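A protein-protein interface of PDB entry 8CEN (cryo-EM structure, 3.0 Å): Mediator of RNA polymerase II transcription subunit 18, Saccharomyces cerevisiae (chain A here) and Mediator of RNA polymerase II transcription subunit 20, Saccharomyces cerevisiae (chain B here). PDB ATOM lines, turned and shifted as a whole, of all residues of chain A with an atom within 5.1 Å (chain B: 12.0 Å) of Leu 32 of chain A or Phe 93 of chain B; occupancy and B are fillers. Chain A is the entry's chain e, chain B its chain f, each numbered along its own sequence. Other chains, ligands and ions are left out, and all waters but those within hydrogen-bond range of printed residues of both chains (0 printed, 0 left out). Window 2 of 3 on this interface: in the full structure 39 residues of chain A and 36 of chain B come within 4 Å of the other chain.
O of Phe 93 of chain B is in hydrogen-bond range of NZ of Lys 221 of chain A, at 2.6 Å. NZ of Lys 221 of chain A lies close to N of Gly 95 of chain B (3.1 Å).
N of Leu 32 of chain A is in hydrogen-bond range of O of Lys 221 of chain A (3.0 Å). O of Ala 90 of chain B lies close to OD1 of Asn 94 of chain B, 2.9 Å away. The backbone NH (N) of Tyr 34 of chain A lies within hydrogen-bond range of the backbone carbonyl oxygen (O) of Gly 219 of chain A (2.8 Å).
Among the printed residues, pairs that only touch across the chains: Leu 32 of chain A with Phe 93 of chain B (3.6 Å), Leu 33 of chain A with Phe 93 of chain B (3.8 Å), Tyr 34 of chain A with Asn 94 of chain B (3.2 Å) and Lys 221 of chain A with Asn 94 of chain B (3.2 Å).
No residue of chain B comes within 4 Å of Pro 30 of chain A. No residue of chain B comes within 4 Å of Pro 31 of chain A. Leu 32 of chain A touches just one residue of chain B: Phe 93. Leu 33 of chain A touches just one residue of chain B: Phe 93. Gly 219 of chain A touches none of the printed residues of chain B. Val 220 of chain A touches none of the printed residues of chain B. No residue of chain B comes within 4 Å of Phe 223 of chain A. Pro 88 of chain B touches none of the printed residues of chain A. Of chain A, only Leu 32 (3.6 Å), Leu 33 (3.8 Å) and Lys 221 (2.6 Å) come within 4 Å of Phe 93 of chain B. Printed residues of chain A within 4 Å of Asn 94 of chain B: Tyr 34 and Lys 221. Printed residues of chain A within 4 Å of Gly 95 of chain B: Lys 221 (3.1 Å). The nearest residue of chain B that does not touch Leu 32 of chain A is Asn 94 of chain B (7.5 Å). The nearest residue of chain A that does not touch Phe 93 of chain B is Phe 223 of chain A (4.5 Å).
Printed residues of chain B that touch a printed residue of chain A: Phe 93, Asn 94 and Gly 95. Of the 9 printed residues of chain A, 4 touch a printed residue of chain B. Among the printed residues, 6 pairs touch across the chains. Among the printed residues, no Asp or Glu carboxylate lies within 4 Å of a Lys or Arg side-chain nitrogen of the other chain.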
ATOM      1  N   PRO A  30     -17.344  -6.090  37.039  1.00  0.00           N
ATOM      2  CA  PRO A  30     -16.247  -7.054  37.096  1.00  0.00           C
ATOM      3  C   PRO A  30     -15.366  -6.946  35.866  1.00  0.00           C
ATOM      4  O   PRO A  30     -15.823  -6.513  34.793  1.00  0.00           O
ATOM      5  CB  PRO A  30     -16.972  -8.413  37.150  1.00  0.00           C
ATOM      6  CG  PRO A  30     -18.370  -8.099  37.568  1.00  0.00           C
ATOM      7  CD  PRO A  30     -18.661  -6.745  37.011  1.00  0.00           C
ATOM      8  N   PRO A  31     -14.087  -7.307  35.975  1.00  0.00           N
ATOM      9  CA  PRO A  31     -13.210  -7.289  34.798  1.00  0.00           C
ATOM     10  C   PRO A  31     -13.614  -8.337  33.772  1.00  0.00           C
ATOM     11  O   PRO A  31     -14.198  -9.373  34.099  1.00  0.00           O
ATOM     12  CB  PRO A  31     -11.826  -7.588  35.384  1.00  0.00           C
ATOM     13  CG  PRO A  31     -12.103  -8.303  36.656  1.00  0.00           C
ATOM     14  CD  PRO A  31     -13.365  -7.705  37.195  1.00  0.00           C
ATOM     15  N   LEU A  32     -13.295  -8.049  32.511  1.00  0.00           N
ATOM     16  CA  LEU A  32     -13.737  -8.855  31.378  1.00  0.00           C
ATOM     17  C   LEU A  32     -12.529  -9.374  30.614  1.00  0.00           C
ATOM     18  O   LEU A  32     -11.876  -8.614  29.892  1.00  0.00           O
ATOM     19  CB  LEU A  32     -14.642  -8.039  30.463  1.00  0.00           C
ATOM     20  CG  LEU A  32     -15.957  -7.660  31.128  1.00  0.00           C
ATOM     21  CD1 LEU A  32     -16.753  -6.738  30.229  1.00  0.00           C
ATOM     22  CD2 LEU A  32     -16.720  -8.931  31.451  1.00  0.00           C
ATOM     23  N   LEU A  33     -12.257 -10.671  30.750  1.00  0.00           N
ATOM     24  CA  LEU A  33     -11.146 -11.294  30.042  1.00  0.00           C
ATOM     25  C   LEU A  33     -11.397 -11.275  28.540  1.00  0.00           C
ATOM     26  O   LEU A  33     -12.480 -11.639  28.073  1.00  0.00           O
ATOM     27  CB  LEU A  33     -10.948 -12.727  30.532  1.00  0.00           C
ATOM     28  CG  LEU A  33      -9.658 -13.448  30.150  1.00  0.00           C
ATOM     29  CD1 LEU A  33      -8.469 -12.878  30.906  1.00  0.00           C
ATOM     30  CD2 LEU A  33      -9.807 -14.935  30.417  1.00  0.00           C
ATOM     31  N   TYR A  34     -10.390 -10.840  27.785  1.00  0.00           N
ATOM     32  CA  TYR A  34     -10.500 -10.700  26.343  1.00  0.00           C
ATOM     33  C   TYR A  34      -9.155 -11.011  25.707  1.00  0.00           C
ATOM     34  O   TYR A  34      -8.113 -10.999  26.366  1.00  0.00           O
ATOM     35  CB  TYR A  34     -10.969  -9.289  25.945  1.00  0.00           C
ATOM     36  CG  TYR A  34      -9.890  -8.223  26.007  1.00  0.00           C
ATOM     37  CD1 TYR A  34      -9.548  -7.626  27.212  1.00  0.00           C
ATOM     38  CD2 TYR A  34      -9.234  -7.796  24.856  1.00  0.00           C
ATOM     39  CE1 TYR A  34      -8.568  -6.650  27.276  1.00  0.00           C
ATOM     40  CE2 TYR A  34      -8.252  -6.822  24.911  1.00  0.00           C
ATOM     41  CZ  TYR A  34      -7.925  -6.253  26.122  1.00  0.00           C
ATOM     42  OH  TYR A  34      -6.953  -5.283  26.181  1.00  0.00           O
ATOM     43  N   GLY A 219      -5.972  -9.803  28.130  1.00  0.00           N
ATOM     44  CA  GLY A 219      -6.136  -8.907  29.249  1.00  0.00           C
ATOM     45  C   GLY A 219      -7.559  -8.871  29.752  1.00  0.00           C
ATOM     46  O   GLY A 219      -8.409  -9.658  29.333  1.00  0.00           O
ATOM     47  N   VAL A 220      -7.797  -7.945  30.677  1.00  0.00           N
ATOM     48  CA  VAL A 220      -9.113  -7.706  31.254  1.00  0.00           C
ATOM     49  C   VAL A 220      -9.455  -6.230  31.100  1.00  0.00           C
ATOM     50  O   VAL A 220      -8.580  -5.364  31.203  1.00  0.00           O
ATOM     51  CB  VAL A 220      -9.183  -8.148  32.733  1.00  0.00           C
ATOM     52  CG1 VAL A 220      -9.070  -9.658  32.838  1.00  0.00           C
ATOM     53  CG2 VAL A 220      -8.073  -7.500  33.543  1.00  0.00           C
ATOM     54  N   LYS A 221     -10.726  -5.939  30.829  1.00  0.00           N
ATOM     55  CA  LYS A 221     -11.158  -4.562  30.643  1.00  0.00           C
ATOM     56  C   LYS A 221     -12.353  -4.241  31.529  1.00  0.00           C
ATOM     57  O   LYS A 221     -13.100  -5.123  31.957  1.00  0.00           O
ATOM     58  CB  LYS A 221     -11.511  -4.251  29.183  1.00  0.00           C
ATOM     59  CG  LYS A 221     -12.698  -5.009  28.633  1.00  0.00           C
ATOM     60  CD  LYS A 221     -12.961  -4.580  27.201  1.00  0.00           C
ATOM     61  CE  LYS A 221     -11.908  -5.124  26.259  1.00  0.00           C
ATOM     62  NZ  LYS A 221     -12.237  -4.812  24.844  1.00  0.00           N
ATOM     63  N   PHE A 223     -15.712  -1.505  31.768  1.00  0.00           N
ATOM     64  CA  PHE A 223     -16.589  -0.518  31.138  1.00  0.00           C
ATOM     65  C   PHE A 223     -17.147   0.361  32.252  1.00  0.00           C
ATOM     66  O   PHE A 223     -18.211   0.092  32.808  1.00  0.00           O
ATOM     67  CB  PHE A 223     -17.701  -1.193  30.343  1.00  0.00           C
ATOM     68  CG  PHE A 223     -17.228  -1.873  29.092  1.00  0.00           C
ATOM     69  CD1 PHE A 223     -16.196  -1.342  28.338  1.00  0.00           C
ATOM     70  CD2 PHE A 223     -17.825  -3.044  28.667  1.00  0.00           C
ATOM     71  CE1 PHE A 223     -15.770  -1.976  27.183  1.00  0.00           C
ATOM     72  CE2 PHE A 223     -17.403  -3.681  27.515  1.00  0.00           C
ATOM     73  CZ  PHE A 223     -16.374  -3.146  26.773  1.00  0.00           C
ATOM     74  N   ALA B  84     -22.860  -0.594  11.909  1.00  0.00           N
ATOM     75  CA  ALA B  84     -22.679  -1.134  13.249  1.00  0.00           C
ATOM     76  C   ALA B  84     -23.673  -2.236  13.591  1.00  0.00           C
ATOM     77  O   ALA B  84     -23.517  -2.886  14.630  1.00  0.00           O
ATOM     78  CB  ALA B  84     -22.785  -0.014  14.289  1.00  0.00           C
ATOM     79  N   ASP B  86     -24.377  -5.091  11.780  1.00  0.00           N
ATOM     80  CA  ASP B  86     -23.943  -6.423  11.384  1.00  0.00           C
ATOM     81  C   ASP B  86     -22.514  -6.742  11.808  1.00  0.00           C
ATOM     82  O   ASP B  86     -21.940  -7.719  11.316  1.00  0.00           O
ATOM     83  CB  ASP B  86     -24.095  -6.597   9.871  1.00  0.00           C
ATOM     84  CG  ASP B  86     -23.521  -5.436   9.089  1.00  0.00           C
ATOM     85  OD1 ASP B  86     -23.529  -4.301   9.611  1.00  0.00           O
ATOM     86  OD2 ASP B  86     -23.063  -5.660   7.950  1.00  0.00           O
ATOM     87  N   ILE B  87     -21.925  -5.941  12.686  1.00  0.00           N
ATOM     88  CA  ILE B  87     -20.645  -6.328  13.293  1.00  0.00           C
ATOM     89  C   ILE B  87     -20.876  -7.521  14.211  1.00  0.00           C
ATOM     90  O   ILE B  87     -21.887  -7.546  14.938  1.00  0.00           O
ATOM     91  CB  ILE B  87     -20.042  -5.154  14.069  1.00  0.00           C
ATOM     92  CG1 ILE B  87     -20.010  -3.886  13.223  1.00  0.00           C
ATOM     93  CG2 ILE B  87     -18.632  -5.485  14.539  1.00  0.00           C
ATOM     94  CD1 ILE B  87     -19.416  -2.709  13.965  1.00  0.00           C
ATOM     95  N   PRO B  88     -20.015  -8.534  14.198  1.00  0.00           N
ATOM     96  CA  PRO B  88     -20.039  -9.537  15.265  1.00  0.00           C
ATOM     97  C   PRO B  88     -19.749  -8.885  16.605  1.00  0.00           C
ATOM     98  O   PRO B  88     -18.883  -8.003  16.695  1.00  0.00           O
ATOM     99  CB  PRO B  88     -18.925 -10.514  14.863  1.00  0.00           C
ATOM    100  CG  PRO B  88     -18.763 -10.321  13.393  1.00  0.00           C
ATOM    101  CD  PRO B  88     -19.042  -8.871  13.144  1.00  0.00           C
ATOM    102  N   PRO B  89     -20.462  -9.279  17.666  1.00  0.00           N
ATOM    103  CA  PRO B  89     -20.215  -8.670  18.985  1.00  0.00           C
ATOM    104  C   PRO B  89     -18.840  -8.973  19.551  1.00  0.00           C
ATOM    105  O   PRO B  89     -18.383  -8.243  20.440  1.00  0.00           O
ATOM    106  CB  PRO B  89     -21.323  -9.270  19.863  1.00  0.00           C
ATOM    107  CG  PRO B  89     -22.366  -9.744  18.896  1.00  0.00           C
ATOM    108  CD  PRO B  89     -21.602 -10.210  17.698  1.00  0.00           C
ATOM    109  N   ALA B  90     -18.175 -10.022  19.063  1.00  0.00           N
ATOM    110  CA  ALA B  90     -16.862 -10.400  19.577  1.00  0.00           C
ATOM    111  C   ALA B  90     -15.811  -9.336  19.279  1.00  0.00           C
ATOM    112  O   ALA B  90     -14.980  -9.024  20.140  1.00  0.00           O
ATOM    113  CB  ALA B  90     -16.448 -11.744  18.988  1.00  0.00           C
ATOM    114  N   LEU B  91     -15.826  -8.773  18.068  1.00  0.00           N
ATOM    115  CA  LEU B  91     -14.838  -7.756  17.717  1.00  0.00           C
ATOM    116  C   LEU B  91     -15.058  -6.464  18.492  1.00  0.00           C
ATOM    117  O   LEU B  91     -14.091  -5.759  18.805  1.00  0.00           O
ATOM    118  CB  LEU B  91     -14.869  -7.485  16.212  1.00  0.00           C
ATOM    119  CG  LEU B  91     -14.443  -8.632  15.293  1.00  0.00           C
ATOM    120  CD1 LEU B  91     -14.275  -8.139  13.865  1.00  0.00           C
ATOM    121  CD2 LEU B  91     -13.167  -9.292  15.789  1.00  0.00           C
ATOM    122  N   VAL B  92     -16.312  -6.131  18.799  1.00  0.00           N
ATOM    123  CA  VAL B  92     -16.591  -4.961  19.625  1.00  0.00           C
ATOM    124  C   VAL B  92     -16.174  -5.214  21.070  1.00  0.00           C
ATOM    125  O   VAL B  92     -15.604  -4.335  21.731  1.00  0.00           O
ATOM    126  CB  VAL B  92     -18.080  -4.580  19.513  1.00  0.00           C
ATOM    127  CG1 VAL B  92     -18.423  -3.425  20.444  1.00  0.00           C
ATOM    128  CG2 VAL B  92     -18.427  -4.226  18.078  1.00  0.00           C
ATOM    129  N   PHE B  93     -16.429  -6.424  21.576  1.00  0.00           N
ATOM    130  CA  PHE B  93     -16.138  -6.724  22.975  1.00  0.00           C
ATOM    131  C   PHE B  93     -14.638  -6.842  23.226  1.00  0.00           C
ATOM    132  O   PHE B  93     -14.150  -6.440  24.287  1.00  0.00           O
ATOM    133  CB  PHE B  93     -16.863  -8.004  23.390  1.00  0.00           C
ATOM    134  CG  PHE B  93     -16.404  -8.568  24.706  1.00  0.00           C
ATOM    135  CD1 PHE B  93     -16.539  -7.836  25.875  1.00  0.00           C
ATOM    136  CD2 PHE B  93     -15.846  -9.833  24.772  1.00  0.00           C
ATOM    137  CE1 PHE B  93     -16.117  -8.355  27.084  1.00  0.00           C
ATOM    138  CE2 PHE B  93     -15.423 -10.358  25.979  1.00  0.00           C
ATOM    139  CZ  PHE B  93     -15.559  -9.618  27.137  1.00  0.00           C
ATOM    140  N   ASN B  94     -13.889  -7.380  22.264  1.00  0.00           N
ATOM    141  CA  ASN B  94     -12.458  -7.587  22.448  1.00  0.00           C
ATOM    142  C   ASN B  94     -11.623  -6.360  22.108  1.00  0.00           C
ATOM    143  O   ASN B  94     -10.392  -6.435  22.168  1.00  0.00           O
ATOM    144  CB  ASN B  94     -11.990  -8.780  21.612  1.00  0.00           C
ATOM    145  CG  ASN B  94     -12.531 -10.101  22.127  1.00  0.00           C
ATOM    146  OD1 ASN B  94     -13.719 -10.227  22.418  1.00  0.00           O
ATOM    147  ND2 ASN B  94     -11.657 -11.092  22.246  1.00  0.00           N
ATOM    148  N   GLY B  95     -12.251  -5.243  21.747  1.00  0.00           N
ATOM    149  CA  GLY B  95     -11.533  -4.008  21.521  1.00  0.00           C
ATOM    150  C   GLY B  95     -10.830  -3.894  20.187  1.00  0.00           C
ATOM    151  O   GLY B  95     -10.119  -2.905  19.968  1.00  0.00           O
ATOM    152  N   SER B  96     -10.990  -4.873  19.294  1.00  0.00           N
ATOM    153  CA  SER B  96     -10.382  -4.768  17.971  1.00  0.00           C
ATOM    154  C   SER B  96     -11.078  -3.705  17.130  1.00  0.00           C
ATOM    155  O   SER B  96     -10.422  -2.962  16.391  1.00  0.00           O
ATOM    156  CB  SER B  96     -10.419  -6.122  17.269  1.00  0.00           C
ATOM    157  OG  SER B  96     -11.743  -6.618  17.195  1.00  0.00           O
ATOM    158  N   SER B  97     -12.399  -3.619  17.228  1.00  0.00           N
ATOM    159  CA  SER B  97     -13.162  -2.591  16.539  1.00  0.00           C
ATOM    160  C   SER B  97     -13.372  -1.386  17.450  1.00  0.00           C
ATOM    161  O   SER B  97     -13.342  -1.489  18.679  1.00  0.00           O
ATOM    162  CB  SER B  97     -14.511  -3.140  16.074  1.00  0.00           C
ATOM    163  OG  SER B  97     -15.336  -2.103  15.572  1.00  0.00           O
ATOM    164  N   THR B  98     -13.588  -0.228  16.826  1.00  0.00           N
ATOM    165  CA  THR B  98     -13.756   1.030  17.542  1.00  0.00           C
ATOM    166  C   THR B  98     -15.205   1.510  17.529  1.00  0.00           C
ATOM    167  O   THR B  98     -15.465   2.715  17.488  1.00  0.00           O
ATOM    168  CB  THR B  98     -12.842   2.104  16.958  1.00  0.00           C
ATOM    169  OG1 THR B  98     -13.327   2.494  15.667  1.00  0.00           O
ATOM    170  CG2 THR B  98     -11.421   1.581  16.821  1.00  0.00           C
ATOM    171  N   GLY B  99     -16.155   0.581  17.563  1.00  0.00           N
ATOM    172  CA  GLY B  99     -17.559   0.939  17.582  1.00  0.00           C
ATOM    173  C   GLY B  99     -18.157   1.191  16.213  1.00  0.00           C
ATOM    174  O   GLY B  99     -18.960   0.387  15.729  1.00  0.00           O
ATOM    175  N   VAL B 100     -17.781   2.293  15.579  1.00  0.00           N
ATOM    176  CA  VAL B 100     -18.320   2.675  14.276  1.00  0.00           C
ATOM    177  C   VAL B 100     -17.253   2.426  13.212  1.00  0.00           C
ATOM    178  O   VAL B 100     -16.107   2.874  13.363  1.00  0.00           O
ATOM    179  CB  VAL B 100     -18.839   4.128  14.266  1.00  0.00           C
ATOM    180  CG1 VAL B 100     -19.985   4.264  15.254  1.00  0.00           C
ATOM    181  CG2 VAL B 100     -17.764   5.144  14.661  1.00  0.00           C
ATOM    182  N   PRO B 101     -17.547   1.640  12.182  1.00  0.00           N
ATOM    183  CA  PRO B 101     -16.581   1.431  11.102  1.00  0.00           C
ATOM    184  C   PRO B 101     -16.593   2.582  10.104  1.00  0.00           C
ATOM    185  O   PRO B 101     -17.370   3.533  10.200  1.00  0.00           O
ATOM    186  CB  PRO B 101     -17.062   0.138  10.437  1.00  0.00           C
ATOM    187  CG  PRO B 101     -17.863  -0.547  11.470  1.00  0.00           C
ATOM    188  CD  PRO B 101     -18.539   0.554  12.237  1.00  0.00           C
